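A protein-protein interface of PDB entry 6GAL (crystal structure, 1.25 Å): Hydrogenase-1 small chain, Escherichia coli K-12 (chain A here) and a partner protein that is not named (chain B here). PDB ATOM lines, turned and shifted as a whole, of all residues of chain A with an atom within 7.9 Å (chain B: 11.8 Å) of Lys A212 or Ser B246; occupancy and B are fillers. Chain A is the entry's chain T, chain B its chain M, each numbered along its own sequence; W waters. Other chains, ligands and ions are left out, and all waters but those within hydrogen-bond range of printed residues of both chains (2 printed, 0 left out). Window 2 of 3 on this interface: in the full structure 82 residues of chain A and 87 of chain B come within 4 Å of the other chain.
The guanidinium group of Arg A192 is in hydrogen-bond range of the backbone carbonyl oxygen of Gly B250 (3.3 Å). The backbone carbonyl oxygen (O) of Gly B250 sits close to the backbone NH (N) of Gly A213 (3.5 Å). O of Arg A211 sits at hydrogen-bond distance from ND2 of Asn B242.
Water W1 lies within hydrogen-bond range of the side-chain hydroxyl of Tyr A191 and the backbone carbonyl oxygen of Val B249. Water W2 bridges the backbone carbonyl oxygen of Gly B250 (2.7 Å) and the guanidinium group of Arg A192 (2.9 Å).
O of Ala B251 sits at hydrogen-bond distance from ND2 of Asn B253, at 3.4 Å. The side-chain amide oxygen (OD1) of Asn B242 lies within hydrogen-bond range of the backbone NH (N) of Asp B244, 3.4 Å away. The side-chain amide nitrogen (ND2) of Asn B242 is in hydrogen-bond range of the backbone carbonyl oxygen (O) of Ser B246, at 3.1 Å. The guanidinium group (NH1) of Arg A192 lies within hydrogen-bond range of the backbone carbonyl oxygen (O) of Tyr A214. ND2 of Asn B242 lies close to N of Ala B248 (3.3 Å). The guanidinium group (NH2) of Arg A192 sits at hydrogen-bond distance from the side-chain hydroxyl (OH) of Tyr A191, at 3.1 Å.
Of chain B, only Ser B246 (3.8 Å) and Gly B247 (3.6 Å) come within 4 Å of Lys A212. Ser B246 touches just one residue of chain A: Lys A212. No residue of chain B comes within 4 Å of Asp A208. No residue of chain B comes within 4 Å of Ala A209. Gly A213 touches just one residue of chain B: Gly B250 (3.2 Å). No residue of chain B comes within 4 Å of Tyr A214. Gly B247 touches two residues of chain A. Of the printed residues of chain A, Asn B242 touches Arg A211. Of the printed residues of chain A, Leu B482 touches Arg A211. Of the printed residues of chain A, Gly B250 touches Arg A192 (3.3 Å) and Gly A213 (3.2 Å). Printed residues of chain B within 4 Å of Arg A192: Gly B250 (3.3 Å). Printed residues of chain A within 4 Å of Ile B241: Arg A211. The nearest residue of chain B that does not touch Lys A212 is Gly B250 (4.1 Å). The nearest residue of chain A that does not touch Ser B246 is Arg A211 (4.7 Å). The nearest printed residue of chain B that does not touch Arg A211 is Ala B240 (4.03 Å).
Ala A210 touches Ala B240 (O to CB, 3.8 Å). O of Ile B241 touches CG of Arg A211 (3.7 Å). Arg A211 touches Gly B247. CB of Ala B251 touches O of Arg A211 (3.6 Å). NH2 of Arg A211 touches C of Leu B482, at 3.9 Å. Lys A212 touches Ser B246 (CG to O, 3.8 Å). CA of Lys A212 touches O of Gly B247, 3.6 Å away.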
ATOM      1  N   TYR A 191      -8.177 -18.861 -30.595  1.00  0.00           N
ATOM      2  CA  TYR A 191      -8.658 -19.026 -29.216  1.00  0.00           C
ATOM      3  C   TYR A 191     -10.161 -18.832 -29.063  1.00  0.00           C
ATOM      4  O   TYR A 191     -10.692 -19.132 -27.983  1.00  0.00           O
ATOM      5  CB  TYR A 191      -7.889 -18.132 -28.216  1.00  0.00           C
ATOM      6  CG  TYR A 191      -8.385 -16.713 -28.115  1.00  0.00           C
ATOM      7  CD1 TYR A 191      -8.562 -15.891 -29.235  1.00  0.00           C
ATOM      8  CD2 TYR A 191      -8.633 -16.141 -26.880  1.00  0.00           C
ATOM      9  CE1 TYR A 191      -9.025 -14.610 -29.124  1.00  0.00           C
ATOM     10  CE2 TYR A 191      -9.097 -14.849 -26.758  1.00  0.00           C
ATOM     11  CZ  TYR A 191      -9.321 -14.072 -27.898  1.00  0.00           C
ATOM     12  OH  TYR A 191      -9.815 -12.789 -27.774  1.00  0.00           O
ATOM     13  N   ARG A 192     -10.878 -18.404 -30.104  1.00  0.00           N
ATOM     14  CA  ARG A 192     -12.362 -18.376 -30.056  1.00  0.00           C
ATOM     15  C   ARG A 192     -13.014 -19.582 -30.667  1.00  0.00           C
ATOM     16  O   ARG A 192     -14.234 -19.625 -30.755  1.00  0.00           O
ATOM     17  CB  ARG A 192     -12.910 -17.063 -30.649  1.00  0.00           C
ATOM     18  CG  ARG A 192     -12.331 -15.838 -29.943  1.00  0.00           C
ATOM     19  CD  ARG A 192     -12.949 -14.511 -30.386  1.00  0.00           C
ATOM     20  NE  ARG A 192     -12.372 -13.389 -29.710  1.00  0.00           N
ATOM     21  CZ  ARG A 192     -12.916 -12.186 -29.545  1.00  0.00           C
ATOM     22  NH1 ARG A 192     -14.141 -11.931 -29.977  1.00  0.00           N
ATOM     23  NH2 ARG A 192     -12.232 -11.278 -28.865  1.00  0.00           N
ATOM     24  N   HIS A 195     -16.049 -21.155 -29.007  1.00  0.00           N
ATOM     25  CA  HIS A 195     -17.320 -20.467 -29.276  1.00  0.00           C
ATOM     26  C   HIS A 195     -17.849 -20.825 -30.648  1.00  0.00           C
ATOM     27  O   HIS A 195     -19.043 -21.071 -30.804  1.00  0.00           O
ATOM     28  CB  HIS A 195     -17.144 -18.959 -29.101  1.00  0.00           C
ATOM     29  CG  HIS A 195     -16.703 -18.580 -27.726  1.00  0.00           C
ATOM     30  ND1 HIS A 195     -17.405 -18.926 -26.584  1.00  0.00           N
ATOM     31  CD2 HIS A 195     -15.620 -17.875 -27.312  1.00  0.00           C
ATOM     32  CE1 HIS A 195     -16.759 -18.432 -25.540  1.00  0.00           C
ATOM     33  NE2 HIS A 195     -15.672 -17.798 -25.949  1.00  0.00           N
ATOM     34  N   GLU A 200     -21.639 -19.974 -30.612  1.00  0.00           N
ATOM     35  CA  GLU A 200     -21.668 -18.804 -29.785  1.00  0.00           C
ATOM     36  C   GLU A 200     -20.989 -17.678 -30.580  1.00  0.00           C
ATOM     37  O   GLU A 200     -19.768 -17.619 -30.667  1.00  0.00           O
ATOM     38  CB  GLU A 200     -20.929 -19.077 -28.481  1.00  0.00           C
ATOM     39  CG  GLU A 200     -21.742 -19.992 -27.575  1.00  0.00           C
ATOM     40  CD  GLU A 200     -21.020 -20.525 -26.370  1.00  0.00           C
ATOM     41  OE1 GLU A 200     -21.690 -21.117 -25.483  1.00  0.00           O
ATOM     42  OE2 GLU A 200     -19.794 -20.379 -26.275  1.00  0.00           O
ATOM     43  N   VAL A 202     -20.837 -13.413 -31.894  1.00  0.00           N
ATOM     44  CA  VAL A 202     -21.176 -12.002 -31.972  1.00  0.00           C
ATOM     45  C   VAL A 202     -22.182 -11.815 -33.128  1.00  0.00           C
ATOM     46  O   VAL A 202     -21.946 -12.302 -34.243  1.00  0.00           O
ATOM     47  CB  VAL A 202     -19.936 -11.145 -32.203  1.00  0.00           C
ATOM     48  CG1 VAL A 202     -20.321  -9.655 -32.347  1.00  0.00           C
ATOM     49  CG2 VAL A 202     -18.950 -11.319 -31.037  1.00  0.00           C
ATOM     50  N   ASP A 207     -22.388  -6.239 -28.611  1.00  0.00           N
ATOM     51  CA  ASP A 207     -23.421  -6.996 -27.959  1.00  0.00           C
ATOM     52  C   ASP A 207     -22.801  -7.796 -26.796  1.00  0.00           C
ATOM     53  O   ASP A 207     -21.581  -7.737 -26.532  1.00  0.00           O
ATOM     54  CB  ASP A 207     -24.256  -7.858 -28.922  1.00  0.00           C
ATOM     55  CG  ASP A 207     -23.498  -9.015 -29.612  1.00  0.00           C
ATOM     56  OD1 ASP A 207     -22.336  -9.264 -29.257  1.00  0.00           O
ATOM     57  OD2 ASP A 207     -24.127  -9.649 -30.546  1.00  0.00           O
ATOM     58  N   ASP A 208     -23.642  -8.498 -26.044  1.00  0.00           N
ATOM     59  CA  ASP A 208     -23.146  -9.208 -24.870  1.00  0.00           C
ATOM     60  C   ASP A 208     -22.133 -10.272 -25.265  1.00  0.00           C
ATOM     61  O   ASP A 208     -21.151 -10.519 -24.556  1.00  0.00           O
ATOM     62  CB  ASP A 208     -24.270  -9.808 -24.055  1.00  0.00           C
ATOM     63  CG  ASP A 208     -25.104  -8.740 -23.330  1.00  0.00           C
ATOM     64  OD1 ASP A 208     -24.702  -7.555 -23.209  1.00  0.00           O
ATOM     65  OD2 ASP A 208     -26.152  -9.102 -22.781  1.00  0.00           O
ATOM     66  N   ALA A 209     -22.373 -10.896 -26.411  1.00  0.00           N
ATOM     67  CA  ALA A 209     -21.451 -11.884 -26.963  1.00  0.00           C
ATOM     68  C   ALA A 209     -20.076 -11.314 -27.254  1.00  0.00           C
ATOM     69  O   ALA A 209     -19.061 -11.904 -26.898  1.00  0.00           O
ATOM     70  CB  ALA A 209     -22.044 -12.489 -28.231  1.00  0.00           C
ATOM     71  N   ALA A 210     -20.059 -10.106 -27.793  1.00  0.00           N
ATOM     72  CA  ALA A 210     -18.800  -9.415 -28.103  1.00  0.00           C
ATOM     73  C   ALA A 210     -18.032  -9.131 -26.833  1.00  0.00           C
ATOM     74  O   ALA A 210     -16.813  -9.256 -26.806  1.00  0.00           O
ATOM     75  CB  ALA A 210     -19.090  -8.118 -28.859  1.00  0.00           C
ATOM     76  N   ARG A 211     -18.737  -8.786 -25.758  1.00  0.00           N
ATOM     77  CA  ARG A 211     -18.116  -8.470 -24.478  1.00  0.00           C
ATOM     78  C   ARG A 211     -17.612  -9.694 -23.719  1.00  0.00           C
ATOM     79  O   ARG A 211     -16.878  -9.530 -22.752  1.00  0.00           O
ATOM     80  CB  ARG A 211     -19.102  -7.669 -23.608  1.00  0.00           C
ATOM     81  CG  ARG A 211     -19.369  -6.293 -24.167  1.00  0.00           C
ATOM     82  CD  ARG A 211     -20.490  -5.580 -23.436  1.00  0.00           C
ATOM     83  NE  ARG A 211     -20.721  -4.247 -24.004  1.00  0.00           N
ATOM     84  CZ  ARG A 211     -21.285  -3.230 -23.346  1.00  0.00           C
ATOM     85  NH1 ARG A 211     -21.826  -3.400 -22.148  1.00  0.00           N
ATOM     86  NH2 ARG A 211     -21.419  -2.073 -23.929  1.00  0.00           N
ATOM     87  N   LYS A 212     -17.938 -10.881 -24.210  1.00  0.00           N
ATOM     88  CA  LYS A 212     -17.412 -12.149 -23.690  1.00  0.00           C
ATOM     89  C   LYS A 212     -16.406 -12.798 -24.626  1.00  0.00           C
ATOM     90  O   LYS A 212     -15.961 -13.900 -24.338  1.00  0.00           O
ATOM     91  CB  LYS A 212     -18.545 -13.158 -23.415  1.00  0.00           C
ATOM     92  CG  LYS A 212     -19.482 -12.774 -22.302  1.00  0.00           C
ATOM     93  CD  LYS A 212     -20.634 -13.780 -22.191  1.00  0.00           C
ATOM     94  CE  LYS A 212     -21.708 -13.579 -23.261  1.00  0.00           C
ATOM     95  NZ  LYS A 212     -22.818 -14.555 -23.086  1.00  0.00           N
ATOM     96  N   GLY A 213     -16.058 -12.137 -25.748  1.00  0.00           N
ATOM     97  CA  GLY A 213     -15.125 -12.696 -26.689  1.00  0.00           C
ATOM     98  C   GLY A 213     -15.638 -13.858 -27.505  1.00  0.00           C
ATOM     99  O   GLY A 213     -14.872 -14.765 -27.851  1.00  0.00           O
ATOM    100  N   TYR A 214     -16.917 -13.842 -27.888  1.00  0.00           N
ATOM    101  CA  TYR A 214     -17.458 -14.877 -28.731  1.00  0.00           C
ATOM    102  C   TYR A 214     -16.899 -14.790 -30.160  1.00  0.00           C
ATOM    103  O   TYR A 214     -16.257 -13.806 -30.569  1.00  0.00           O
ATOM    104  CB  TYR A 214     -18.984 -14.859 -28.725  1.00  0.00           C
ATOM    105  CG  TYR A 214     -19.663 -15.443 -27.486  1.00  0.00           C
ATOM    106  CD1 TYR A 214     -18.958 -15.778 -26.326  1.00  0.00           C
ATOM    107  CD2 TYR A 214     -21.029 -15.659 -27.503  1.00  0.00           C
ATOM    108  CE1 TYR A 214     -19.620 -16.314 -25.215  1.00  0.00           C
ATOM    109  CE2 TYR A 214     -21.705 -16.179 -26.400  1.00  0.00           C
ATOM    110  CZ  TYR A 214     -20.987 -16.497 -25.267  1.00  0.00           C
ATOM    111  OH  TYR A 214     -21.620 -17.014 -24.179  1.00  0.00           O
ATOM    112  N   CYS A 215     -17.134 -15.860 -30.903  1.00  0.00           N
ATOM    113  CA  CYS A 215     -16.636 -16.013 -32.250  1.00  0.00           C
ATOM    114  C   CYS A 215     -17.193 -14.961 -33.182  1.00  0.00           C
ATOM    115  O   CYS A 215     -18.319 -14.535 -33.038  1.00  0.00           O
ATOM    116  CB  CYS A 215     -16.872 -17.426 -32.751  1.00  0.00           C
ATOM    117  SG  CYS A 215     -16.587 -17.692 -34.529  1.00  0.00           S
ATOM    118  N   PRO B 238     -14.365  -1.862 -32.655  1.00  0.00           N
ATOM    119  CA  PRO B 238     -14.761  -3.249 -32.386  1.00  0.00           C
ATOM    120  C   PRO B 238     -14.243  -3.809 -31.064  1.00  0.00           C
ATOM    121  O   PRO B 238     -14.602  -4.926 -30.714  1.00  0.00           O
ATOM    122  CB  PRO B 238     -14.172  -4.017 -33.583  1.00  0.00           C
ATOM    123  CG  PRO B 238     -13.169  -3.164 -34.168  1.00  0.00           C
ATOM    124  CD  PRO B 238     -13.237  -1.790 -33.599  1.00  0.00           C
ATOM    125  N   CYS B 239     -13.412  -3.055 -30.357  1.00  0.00           N
ATOM    126  CA  CYS B 239     -12.769  -3.533 -29.149  1.00  0.00           C
ATOM    127  C   CYS B 239     -13.686  -3.364 -27.929  1.00  0.00           C
ATOM    128  O   CYS B 239     -13.522  -2.475 -27.092  1.00  0.00           O
ATOM    129  CB  CYS B 239     -11.428  -2.821 -28.961  1.00  0.00           C
ATOM    130  SG  CYS B 239     -11.543  -1.008 -29.042  1.00  0.00           S
ATOM    131  N   ALA B 240     -14.659  -4.262 -27.855  1.00  0.00           N
ATOM    132  CA  ALA B 240     -15.636  -4.279 -26.760  1.00  0.00           C
ATOM    133  C   ALA B 240     -14.902  -4.375 -25.426  1.00  0.00           C
ATOM    134  O   ALA B 240     -13.848  -5.033 -25.305  1.00  0.00           O
ATOM    135  CB  ALA B 240     -16.563  -5.466 -26.935  1.00  0.00           C
ATOM    136  N   ILE B 241     -15.490  -3.689 -24.449  1.00  0.00           N
ATOM    137  CA  ILE B 241     -14.918  -3.572 -23.126  1.00  0.00           C
ATOM    138  C   ILE B 241     -15.714  -4.415 -22.125  1.00  0.00           C
ATOM    139  O   ILE B 241     -16.956  -4.426 -22.138  1.00  0.00           O
ATOM    140  CB  ILE B 241     -14.911  -2.092 -22.681  1.00  0.00           C
ATOM    141  CG1 ILE B 241     -14.044  -1.281 -23.617  1.00  0.00           C
ATOM    142  CG2 ILE B 241     -14.429  -1.928 -21.245  1.00  0.00           C
ATOM    143  CD1 ILE B 241     -14.108   0.221 -23.444  1.00  0.00           C
ATOM    144  N   ASN B 242     -14.976  -5.063 -21.209  1.00  0.00           N
ATOM    145  CA  ASN B 242     -15.588  -5.792 -20.097  1.00  0.00           C
ATOM    146  C   ASN B 242     -14.558  -5.766 -18.998  1.00  0.00           C
ATOM    147  O   ASN B 242     -13.483  -6.358 -19.127  1.00  0.00           O
ATOM    148  CB  ASN B 242     -15.914  -7.211 -20.561  1.00  0.00           C
ATOM    149  CG  ASN B 242     -16.505  -8.075 -19.469  1.00  0.00           C
ATOM    150  OD1 ASN B 242     -16.489  -7.709 -18.279  1.00  0.00           O
ATOM    151  ND2 ASN B 242     -16.925  -9.278 -19.855  1.00  0.00           N
ATOM    152  N   ILE B 243     -14.881  -5.069 -17.927  1.00  0.00           N
ATOM    153  CA  ILE B 243     -13.973  -4.928 -16.781  1.00  0.00           C
ATOM    154  C   ILE B 243     -14.283  -5.922 -15.672  1.00  0.00           C
ATOM    155  O   ILE B 243     -13.368  -6.428 -15.035  1.00  0.00           O
ATOM    156  CB  ILE B 243     -14.032  -3.509 -16.186  1.00  0.00           C
ATOM    157  CG1 ILE B 243     -13.854  -2.448 -17.261  1.00  0.00           C
ATOM    158  CG2 ILE B 243     -12.966  -3.333 -15.123  1.00  0.00           C
ATOM    159  CD1 ILE B 243     -12.568  -2.615 -18.038  1.00  0.00           C
ATOM    160  N   ASP B 244     -15.544  -6.134 -15.363  1.00  0.00           N
ATOM    161  CA  ASP B 244     -15.934  -6.789 -14.092  1.00  0.00           C
ATOM    162  C   ASP B 244     -16.957  -7.909 -14.241  1.00  0.00           C
ATOM    163  O   ASP B 244     -17.623  -8.286 -13.263  1.00  0.00           O
ATOM    164  CB  ASP B 244     -16.416  -5.729 -13.082  1.00  0.00           C
ATOM    165  CG  ASP B 244     -16.538  -6.220 -11.640  1.00  0.00           C
ATOM    166  OD1 ASP B 244     -15.678  -7.004 -11.153  1.00  0.00           O
ATOM    167  OD2 ASP B 244     -17.518  -5.818 -10.963  1.00  0.00           O
ATOM    168  N   GLU B 245     -17.102  -8.442 -15.442  1.00  0.00           N
ATOM    169  CA  GLU B 245     -18.064  -9.493 -15.690  1.00  0.00           C
ATOM    170  C   GLU B 245     -17.375 -10.731 -16.206  1.00  0.00           C
ATOM    171  O   GLU B 245     -16.252 -10.670 -16.705  1.00  0.00           O
ATOM    172  CB  GLU B 245     -19.155  -9.043 -16.667  1.00  0.00           C
ATOM    173  CG  GLU B 245     -19.986  -7.864 -16.170  1.00  0.00           C
ATOM    174  CD  GLU B 245     -20.550  -7.070 -17.353  1.00  0.00           C
ATOM    175  OE1 GLU B 245     -21.525  -7.593 -17.887  1.00  0.00           O
ATOM    176  OE2 GLU B 245     -20.002  -5.971 -17.796  1.00  0.00           O
ATOM    177  N   SER B 246     -18.055 -11.863 -16.109  1.00  0.00           N
ATOM    178  CA  SER B 246     -17.572 -13.090 -16.714  1.00  0.00           C
ATOM    179  C   SER B 246     -17.206 -12.841 -18.194  1.00  0.00           C
ATOM    180  O   SER B 246     -17.893 -12.119 -18.919  1.00  0.00           O
ATOM    181  CB  SER B 246     -18.608 -14.198 -16.581  1.00  0.00           C
ATOM    182  OG  SER B 246     -18.102 -15.417 -17.056  1.00  0.00           O
ATOM    183  N   GLY B 247     -16.142 -13.475 -18.629  1.00  0.00           N
ATOM    184  CA  GLY B 247     -15.729 -13.317 -19.989  1.00  0.00           C
ATOM    185  C   GLY B 247     -14.895 -12.086 -20.277  1.00  0.00           C
ATOM    186  O   GLY B 247     -14.584 -11.859 -21.461  1.00  0.00           O
ATOM    187  N   ALA B 248     -14.423 -11.386 -19.250  1.00  0.00           N
ATOM    188  CA  ALA B 248     -13.567 -10.228 -19.496  1.00  0.00           C
ATOM    189  C   ALA B 248     -12.262 -10.621 -20.165  1.00  0.00           C
ATOM    190  O   ALA B 248     -11.641  -9.798 -20.841  1.00  0.00           O
ATOM    191  CB  ALA B 248     -13.275  -9.479 -18.233  1.00  0.00           C
ATOM    192  N   VAL B 249     -11.902 -11.912 -20.035  1.00  0.00           N
ATOM    193  CA  VAL B 249     -10.757 -12.446 -20.754  1.00  0.00           C
ATOM    194  C   VAL B 249     -10.911 -12.319 -22.274  1.00  0.00           C
ATOM    195  O   VAL B 249      -9.903 -12.443 -22.988  1.00  0.00           O
ATOM    196  CB  VAL B 249     -10.481 -13.916 -20.430  1.00  0.00           C
ATOM    197  CG1 VAL B 249      -9.996 -14.020 -18.987  1.00  0.00           C
ATOM    198  CG2 VAL B 249     -11.656 -14.843 -20.667  1.00  0.00           C
ATOM    199  N   GLY B 250     -12.138 -12.134 -22.773  1.00  0.00           N
ATOM    200  CA  GLY B 250     -12.371 -11.978 -24.190  1.00  0.00           C
ATOM    201  C   GLY B 250     -12.556 -10.554 -24.664  1.00  0.00           C
ATOM    202  O   GLY B 250     -13.095 -10.363 -25.775  1.00  0.00           O
ATOM    203  N   ALA B 251     -12.132  -9.591 -23.871  1.00  0.00           N
ATOM    204  CA  ALA B 251     -12.440  -8.202 -24.145  1.00  0.00           C
ATOM    205  C   ALA B 251     -11.349  -7.283 -23.629  1.00  0.00           C
ATOM    206  O   ALA B 251     -10.376  -7.727 -23.023  1.00  0.00           O
ATOM    207  CB  ALA B 251     -13.796  -7.873 -23.522  1.00  0.00           C
ATOM    208  N   VAL B 252     -11.487  -5.978 -23.835  1.00  0.00           N
ATOM    209  CA  VAL B 252     -10.613  -5.006 -23.224  1.00  0.00           C
ATOM    210  C   VAL B 252     -10.969  -4.941 -21.737  1.00  0.00           C
ATOM    211  O   VAL B 252     -12.043  -4.511 -21.359  1.00  0.00           O
ATOM    212  CB  VAL B 252     -10.769  -3.618 -23.866  1.00  0.00           C
ATOM    213  CG1 VAL B 252      -9.961  -2.585 -23.127  1.00  0.00           C
ATOM    214  CG2 VAL B 252     -10.336  -3.637 -25.326  1.00  0.00           C
ATOM    215  N   ASN B 253     -10.041  -5.435 -20.923  1.00  0.00           N
ATOM    216  CA  ASN B 253     -10.224  -5.637 -19.475  1.00  0.00           C
ATOM    217  C   ASN B 253      -9.168  -4.815 -18.727  1.00  0.00           C
ATOM    218  O   ASN B 253      -8.419  -4.052 -19.329  1.00  0.00           O
ATOM    219  CB  ASN B 253     -10.190  -7.138 -19.166  1.00  0.00           C
ATOM    220  CG  ASN B 253      -8.879  -7.764 -19.538  1.00  0.00           C
ATOM    221  OD1 ASN B 253      -7.848  -7.171 -19.253  1.00  0.00           O
ATOM    222  ND2 ASN B 253      -8.910  -8.956 -20.165  1.00  0.00           N
ATOM    223  N   MET B 254      -9.166  -4.919 -17.403  1.00  0.00           N
ATOM    224  CA  MET B 254      -8.228  -4.134 -16.602  1.00  0.00           C
ATOM    225  C   MET B 254      -6.765  -4.424 -16.971  1.00  0.00           C
ATOM    226  O   MET B 254      -5.942  -3.520 -16.942  1.00  0.00           O
ATOM    227  CB  MET B 254      -8.460  -4.362 -15.107  1.00  0.00           C
ATOM    228  CG  MET B 254      -7.604  -3.543 -14.147  1.00  0.00           C
ATOM    229  SD  MET B 254      -8.094  -1.830 -13.915  1.00  0.00           S
ATOM    230  CE  MET B 254      -9.644  -1.892 -14.796  1.00  0.00           C
ATOM    231  N   LEU B 482     -19.714   1.757 -20.677  1.00  0.00           N
ATOM    232  CA  LEU B 482     -18.806   0.837 -21.399  1.00  0.00           C
ATOM    233  C   LEU B 482     -18.956   0.839 -22.920  1.00  0.00           C
ATOM    234  O   LEU B 482     -18.100   0.297 -23.619  1.00  0.00           O
ATOM    235  CB  LEU B 482     -18.961  -0.612 -20.949  1.00  0.00           C
ATOM    236  CG  LEU B 482     -18.131  -1.033 -19.727  1.00  0.00           C
ATOM    237  CD1 LEU B 482     -18.147  -0.135 -18.516  1.00  0.00           C
ATOM    238  CD2 LEU B 482     -18.536  -2.470 -19.349  1.00  0.00           C
ATOM    239  N   THR B 484     -18.997   0.928 -26.811  1.00  0.00           N
ATOM    240  CA  THR B 484     -17.976   1.208 -27.827  1.00  0.00           C
ATOM    241  C   THR B 484     -18.498   1.197 -29.260  1.00  0.00           C
ATOM    242  O   THR B 484     -17.760   1.543 -30.172  1.00  0.00           O
ATOM    243  CB  THR B 484     -16.805   0.204 -27.752  1.00  0.00           C
ATOM    244  OG1 THR B 484     -17.308  -1.133 -27.661  1.00  0.00           O
ATOM    245  CG2 THR B 484     -15.871   0.535 -26.595  1.00  0.00           C
HETATM  246  O   HOH W   1      -9.148 -11.721 -25.465  1.00  0.00           O
HETATM  247  O   HOH W   2     -13.205  -8.719 -27.909  1.00  0.00           O
